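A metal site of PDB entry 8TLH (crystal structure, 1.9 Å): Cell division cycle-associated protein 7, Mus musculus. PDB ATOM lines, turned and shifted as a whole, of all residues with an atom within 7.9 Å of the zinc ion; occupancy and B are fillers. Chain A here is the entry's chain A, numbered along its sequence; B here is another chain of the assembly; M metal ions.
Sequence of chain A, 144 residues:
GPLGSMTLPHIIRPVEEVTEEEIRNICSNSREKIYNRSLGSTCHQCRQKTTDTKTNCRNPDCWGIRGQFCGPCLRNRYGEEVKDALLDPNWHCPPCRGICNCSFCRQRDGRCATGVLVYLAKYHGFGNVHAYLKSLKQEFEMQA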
ATOM      1  N   SER A  30      21.457  19.782 -23.756  1.00  0.00           N
ATOM      2  CA  SER A  30      22.850  20.233 -23.721  1.00  0.00           C
ATOM      3  C   SER A  30      23.365  20.672 -25.088  1.00  0.00           C
ATOM      4  O   SER A  30      24.318  21.453 -25.142  1.00  0.00           O
ATOM      5  CB  SER A  30      23.737  19.124 -23.162  1.00  0.00           C
ATOM      6  OG  SER A  30      23.693  17.965 -23.973  1.00  0.00           O
ATOM      7  N   LYS A  33      23.259  24.597 -25.689  1.00  0.00           N
ATOM      8  CA  LYS A  33      24.008  25.509 -24.835  1.00  0.00           C
ATOM      9  C   LYS A  33      24.762  26.544 -25.659  1.00  0.00           C
ATOM     10  O   LYS A  33      25.214  26.280 -26.768  1.00  0.00           O
ATOM     11  CB  LYS A  33      24.986  24.724 -23.967  1.00  0.00           C
ATOM     12  CG  LYS A  33      24.323  23.862 -22.900  1.00  0.00           C
ATOM     13  CD  LYS A  33      25.371  23.201 -22.016  1.00  0.00           C
ATOM     14  CE  LYS A  33      24.725  22.443 -20.876  1.00  0.00           C
ATOM     15  NZ  LYS A  33      25.749  21.812 -19.993  1.00  0.00           N
ATOM     16  N   THR A  42      30.292  27.693 -15.310  1.00  0.00           N
ATOM     17  CA  THR A  42      30.725  26.319 -15.495  1.00  0.00           C
ATOM     18  C   THR A  42      29.860  25.378 -14.663  1.00  0.00           C
ATOM     19  O   THR A  42      29.668  25.601 -13.468  1.00  0.00           O
ATOM     20  CB  THR A  42      32.200  26.170 -15.097  1.00  0.00           C
ATOM     21  OG1 THR A  42      32.991  27.090 -15.862  1.00  0.00           O
ATOM     22  CG2 THR A  42      32.685  24.742 -15.365  1.00  0.00           C
ATOM     23  N   CYS A  43      29.343  24.339 -15.314  1.00  0.00           N
ATOM     24  CA  CYS A  43      28.691  23.257 -14.603  1.00  0.00           C
ATOM     25  C   CYS A  43      29.757  22.316 -14.050  1.00  0.00           C
ATOM     26  O   CYS A  43      30.662  21.896 -14.769  1.00  0.00           O
ATOM     27  CB  CYS A  43      27.751  22.504 -15.547  1.00  0.00           C
ATOM     28  SG  CYS A  43      27.113  20.920 -14.922  1.00  0.00           S
ATOM     29  N   HIS A  44      29.645  21.994 -12.755  1.00  0.00           N
ATOM     30  CA  HIS A  44      30.636  21.108 -12.140  1.00  0.00           C
ATOM     31  C   HIS A  44      30.661  19.746 -12.820  1.00  0.00           C
ATOM     32  O   HIS A  44      31.734  19.136 -12.955  1.00  0.00           O
ATOM     33  CB  HIS A  44      30.339  20.950 -10.649  1.00  0.00           C
ATOM     34  CG  HIS A  44      31.172  19.892  -9.983  1.00  0.00           C
ATOM     35  ND1 HIS A  44      32.516  20.052  -9.726  1.00  0.00           N
ATOM     36  CD2 HIS A  44      30.841  18.673  -9.516  1.00  0.00           C
ATOM     37  CE1 HIS A  44      32.984  18.963  -9.134  1.00  0.00           C
ATOM     38  NE2 HIS A  44      31.985  18.115  -8.989  1.00  0.00           N
ATOM     39  N   GLN A  45      29.502  19.251 -13.255  1.00  0.00           N
ATOM     40  CA  GLN A  45      29.415  17.879 -13.764  1.00  0.00           C
ATOM     41  C   GLN A  45      30.073  17.764 -15.137  1.00  0.00           C
ATOM     42  O   GLN A  45      31.006  16.977 -15.323  1.00  0.00           O
ATOM     43  CB  GLN A  45      27.958  17.436 -13.810  1.00  0.00           C
ATOM     44  CG  GLN A  45      27.755  15.956 -14.112  1.00  0.00           C
ATOM     45  CD  GLN A  45      27.923  15.079 -12.890  1.00  0.00           C
ATOM     46  OE1 GLN A  45      27.955  15.561 -11.748  1.00  0.00           O
ATOM     47  NE2 GLN A  45      28.024  13.773 -13.108  1.00  0.00           N
ATOM     48  N   CYS A  46      29.575  18.516 -16.119  1.00  0.00           N
ATOM     49  CA  CYS A  46      30.070  18.423 -17.492  1.00  0.00           C
ATOM     50  C   CYS A  46      31.229  19.381 -17.788  1.00  0.00           C
ATOM     51  O   CYS A  46      31.829  19.275 -18.861  1.00  0.00           O
ATOM     52  CB  CYS A  46      28.928  18.679 -18.478  1.00  0.00           C
ATOM     53  SG  CYS A  46      28.223  20.338 -18.419  1.00  0.00           S
ATOM     54  N   ARG A  47      31.543  20.294 -16.867  1.00  0.00           N
ATOM     55  CA  ARG A  47      32.705  21.176 -16.971  1.00  0.00           C
ATOM     56  C   ARG A  47      32.661  22.030 -18.241  1.00  0.00           C
ATOM     57  O   ARG A  47      33.686  22.313 -18.856  1.00  0.00           O
ATOM     58  CB  ARG A  47      34.003  20.381 -16.883  1.00  0.00           C
ATOM     59  CG  ARG A  47      34.072  19.529 -15.616  1.00  0.00           C
ATOM     60  CD  ARG A  47      35.443  18.907 -15.413  1.00  0.00           C
ATOM     61  NE  ARG A  47      35.694  17.796 -16.320  1.00  0.00           N
ATOM     62  CZ  ARG A  47      35.437  16.529 -16.042  1.00  0.00           C
ATOM     63  NH1 ARG A  47      34.904  16.177 -14.882  1.00  0.00           N
ATOM     64  NH2 ARG A  47      35.702  15.598 -16.952  1.00  0.00           N
ATOM     65  N   GLN A  48      31.457  22.464 -18.627  1.00  0.00           N
ATOM     66  CA  GLN A  48      31.253  23.361 -19.749  1.00  0.00           C
ATOM     67  C   GLN A  48      30.811  24.720 -19.221  1.00  0.00           C
ATOM     68  O   GLN A  48      29.910  24.800 -18.388  1.00  0.00           O
ATOM     69  CB  GLN A  48      30.205  22.804 -20.708  1.00  0.00           C
ATOM     70  CG  GLN A  48      30.463  21.363 -21.132  1.00  0.00           C
ATOM     71  CD  GLN A  48      31.760  21.195 -21.885  1.00  0.00           C
ATOM     72  OE1 GLN A  48      31.888  21.634 -23.027  1.00  0.00           O
ATOM     73  NE2 GLN A  48      32.744  20.570 -21.246  1.00  0.00           N
ATOM     74  N   THR A  50      28.915  27.843 -19.904  1.00  0.00           N
ATOM     75  CA  THR A  50      27.850  28.286 -20.802  1.00  0.00           C
ATOM     76  C   THR A  50      26.940  29.264 -20.055  1.00  0.00           C
ATOM     77  O   THR A  50      27.024  29.422 -18.841  1.00  0.00           O
ATOM     78  CB  THR A  50      27.034  27.101 -21.322  1.00  0.00           C
ATOM     79  OG1 THR A  50      26.502  26.360 -20.216  1.00  0.00           O
ATOM     80  CG2 THR A  50      27.892  26.193 -22.185  1.00  0.00           C
ATOM     81  N   ASP A  52      23.581  29.267 -19.767  1.00  0.00           N
ATOM     82  CA  ASP A  52      22.307  28.820 -19.210  1.00  0.00           C
ATOM     83  C   ASP A  52      22.335  28.881 -17.686  1.00  0.00           C
ATOM     84  O   ASP A  52      23.391  28.833 -17.055  1.00  0.00           O
ATOM     85  CB  ASP A  52      21.974  27.402 -19.675  1.00  0.00           C
ATOM     86  CG  ASP A  52      23.151  26.458 -19.559  1.00  0.00           C
ATOM     87  OD1 ASP A  52      24.109  26.614 -20.343  1.00  0.00           O
ATOM     88  OD2 ASP A  52      23.125  25.564 -18.686  1.00  0.00           O
ATOM     89  N   LYS A  54      22.164  27.938 -13.864  1.00  0.00           N
ATOM     90  CA  LYS A  54      22.681  26.797 -13.133  1.00  0.00           C
ATOM     91  C   LYS A  54      22.362  26.951 -11.649  1.00  0.00           C
ATOM     92  O   LYS A  54      21.983  28.021 -11.175  1.00  0.00           O
ATOM     93  CB  LYS A  54      24.186  26.628 -13.356  1.00  0.00           C
ATOM     94  CG  LYS A  54      24.543  26.433 -14.824  1.00  0.00           C
ATOM     95  CD  LYS A  54      26.016  26.199 -15.045  1.00  0.00           C
ATOM     96  CE  LYS A  54      26.300  25.970 -16.525  1.00  0.00           C
ATOM     97  NZ  LYS A  54      25.970  27.177 -17.337  1.00  0.00           N
ATOM     98  N   GLN A  68      27.554  24.422  -8.848  1.00  0.00           N
ATOM     99  CA  GLN A  68      26.866  24.877 -10.050  1.00  0.00           C
ATOM    100  C   GLN A  68      26.645  23.697 -10.987  1.00  0.00           C
ATOM    101  O   GLN A  68      27.606  23.078 -11.463  1.00  0.00           O
ATOM    102  CB  GLN A  68      27.674  25.973 -10.760  1.00  0.00           C
ATOM    103  CG  GLN A  68      27.999  27.169  -9.872  1.00  0.00           C
ATOM    104  CD  GLN A  68      28.863  28.193 -10.573  1.00  0.00           C
ATOM    105  OE1 GLN A  68      29.235  28.027 -11.739  1.00  0.00           O
ATOM    106  NE2 GLN A  68      29.194  29.268  -9.864  1.00  0.00           N
ATOM    107  N   PHE A  69      25.379  23.402 -11.276  1.00  0.00           N
ATOM    108  CA  PHE A  69      24.998  22.305 -12.152  1.00  0.00           C
ATOM    109  C   PHE A  69      24.001  22.797 -13.177  1.00  0.00           C
ATOM    110  O   PHE A  69      23.075  23.546 -12.851  1.00  0.00           O
ATOM    111  CB  PHE A  69      24.396  21.133 -11.357  1.00  0.00           C
ATOM    112  CG  PHE A  69      25.403  20.367 -10.543  1.00  0.00           C
ATOM    113  CD1 PHE A  69      25.838  20.839  -9.310  1.00  0.00           C
ATOM    114  CD2 PHE A  69      25.919  19.157 -11.001  1.00  0.00           C
ATOM    115  CE1 PHE A  69      26.762  20.133  -8.570  1.00  0.00           C
ATOM    116  CE2 PHE A  69      26.843  18.451 -10.261  1.00  0.00           C
ATOM    117  CZ  PHE A  69      27.271  18.945  -9.038  1.00  0.00           C
ATOM    118  N   CYS A  70      24.183  22.363 -14.426  1.00  0.00           N
ATOM    119  CA  CYS A  70      23.237  22.710 -15.477  1.00  0.00           C
ATOM    120  C   CYS A  70      22.007  21.821 -15.401  1.00  0.00           C
ATOM    121  O   CYS A  70      21.972  20.806 -14.686  1.00  0.00           O
ATOM    122  CB  CYS A  70      23.906  22.600 -16.856  1.00  0.00           C
ATOM    123  SG  CYS A  70      24.342  20.917 -17.372  1.00  0.00           S
ATOM    124  N   GLY A  71      20.965  22.206 -16.133  1.00  0.00           N
ATOM    125  CA  GLY A  71      19.718  21.490 -16.158  1.00  0.00           C
ATOM    126  C   GLY A  71      19.852  20.018 -16.530  1.00  0.00           C
ATOM    127  O   GLY A  71      19.490  19.122 -15.751  1.00  0.00           O
ATOM    128  N   PRO A  72      20.361  19.741 -17.730  1.00  0.00           N
ATOM    129  CA  PRO A  72      20.506  18.340 -18.150  1.00  0.00           C
ATOM    130  C   PRO A  72      21.348  17.502 -17.209  1.00  0.00           C
ATOM    131  O   PRO A  72      20.983  16.367 -16.905  1.00  0.00           O
ATOM    132  CB  PRO A  72      21.160  18.453 -19.532  1.00  0.00           C
ATOM    133  CG  PRO A  72      20.744  19.794 -20.028  1.00  0.00           C
ATOM    134  CD  PRO A  72      20.714  20.679 -18.821  1.00  0.00           C
ATOM    135  N   CYS A  73      22.457  18.046 -16.703  1.00  0.00           N
ATOM    136  CA  CYS A  73      23.320  17.270 -15.827  1.00  0.00           C
ATOM    137  C   CYS A  73      22.613  16.947 -14.509  1.00  0.00           C
ATOM    138  O   CYS A  73      22.638  15.803 -14.049  1.00  0.00           O
ATOM    139  CB  CYS A  73      24.636  18.008 -15.577  1.00  0.00           C
ATOM    140  SG  CYS A  73      25.930  17.707 -16.815  1.00  0.00           S
ATOM    141  N   LEU A  74      21.970  17.946 -13.908  1.00  0.00           N
ATOM    142  CA  LEU A  74      21.271  17.701 -12.650  1.00  0.00           C
ATOM    143  C   LEU A  74      20.167  16.671 -12.832  1.00  0.00           C
ATOM    144  O   LEU A  74      20.056  15.725 -12.044  1.00  0.00           O
ATOM    145  CB  LEU A  74      20.708  19.011 -12.093  1.00  0.00           C
ATOM    146  CG  LEU A  74      20.300  18.941 -10.615  1.00  0.00           C
ATOM    147  CD1 LEU A  74      21.530  18.777  -9.736  1.00  0.00           C
ATOM    148  CD2 LEU A  74      19.512  20.183 -10.210  1.00  0.00           C
ATOM    149  N   ARG A  77      21.803  13.050 -13.819  1.00  0.00           N
ATOM    150  CA  ARG A  77      22.716  12.408 -12.880  1.00  0.00           C
ATOM    151  C   ARG A  77      22.215  12.400 -11.448  1.00  0.00           C
ATOM    152  O   ARG A  77      22.779  11.677 -10.623  1.00  0.00           O
ATOM    153  CB  ARG A  77      24.080  13.108 -12.923  1.00  0.00           C
ATOM    154  CG  ARG A  77      24.624  13.327 -14.332  1.00  0.00           C
ATOM    155  CD  ARG A  77      25.089  12.037 -14.974  1.00  0.00           C
ATOM    156  NE  ARG A  77      26.256  11.493 -14.299  1.00  0.00           N
ATOM    157  CZ  ARG A  77      27.045  10.561 -14.806  1.00  0.00           C
ATOM    158  NH1 ARG A  77      26.826  10.028 -15.996  1.00  0.00           N
ATOM    159  NH2 ARG A  77      28.095  10.143 -14.098  1.00  0.00           N
ATOM    160  P    DT B  11      25.446  12.093 -19.059  1.00  0.00           P
ATOM    161  OP1  DT B  11      25.290  10.900 -18.197  1.00  0.00           O
ATOM    162  OP2  DT B  11      25.050  13.418 -18.554  1.00  0.00           O
ATOM    163  O5'  DT B  11      26.970  12.160 -19.537  1.00  0.00           O
ATOM    164  C5'  DT B  11      27.572  11.011 -20.099  1.00  0.00           C
ATOM    165  C4'  DT B  11      29.001  11.303 -20.522  1.00  0.00           C
ATOM    166  O4'  DT B  11      28.987  12.287 -21.578  1.00  0.00           O
ATOM    167  C3'  DT B  11      29.871  11.890 -19.439  1.00  0.00           C
ATOM    168  O3'  DT B  11      30.463  10.843 -18.679  1.00  0.00           O
ATOM    169  C2'  DT B  11      30.922  12.670 -20.235  1.00  0.00           C
ATOM    170  C1'  DT B  11      30.189  13.036 -21.530  1.00  0.00           C
ATOM    171  N1   DT B  11      29.849  14.475 -21.650  1.00  0.00           N
ATOM    172  C2   DT B  11      30.802  15.357 -22.098  1.00  0.00           C
ATOM    173  O2   DT B  11      31.930  15.009 -22.397  1.00  0.00           O
ATOM    174  N3   DT B  11      30.392  16.657 -22.175  1.00  0.00           N
ATOM    175  C4   DT B  11      29.150  17.159 -21.861  1.00  0.00           C
ATOM    176  O4   DT B  11      28.868  18.351 -21.967  1.00  0.00           O
ATOM    177  C5   DT B  11      28.185  16.186 -21.397  1.00  0.00           C
ATOM    178  C7   DT B  11      26.800  16.610 -21.025  1.00  0.00           C
ATOM    179  C6   DT B  11      28.583  14.903 -21.314  1.00  0.00           C
HETATM  180 ZN    ZN M   1      26.448  20.010 -16.965  1.00  0.00          ZN
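SG of Cys 46 sits close to NZ of Lys 33, 3.3 Å away. The backbone NH of Gln 45 sits close to the side-chain sulfur of Cys 43, 3.4 Å away. The side-chain sulfur (SG) of Cys 70 lies close to the side-chain amino group (NZ) of Lys 33, at 3.1 Å. The backbone carbonyl oxygen of Gln 48 lies within hydrogen-bond range of the backbone NH of Cys 43, 3.2 Å away. The side-chain amide nitrogen of Gln 48 lies within hydrogen-bond range of the backbone carbonyl oxygen of Cys 46 (2.9 Å).
Lys 33 touches the zinc ion. Of the 21 residues printed, 5 come within 4 Å of the zinc ion. The nearest printed residue that does not touch the zinc ion is Gln 45 (4.3 Å).
The side-chain sulfur (SG) of Cys 46 is bound to the zinc ion. The side-chain sulfur (SG) of Cys 70 is bound to the zinc ion, 2.3 Å away. The zinc ion is bound by SG of Cys 43, 2.3 Å away. The zinc ion is bound by SG of Cys 73, at 2.4 Å. The zinc ion has four donor atoms within binding distance.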
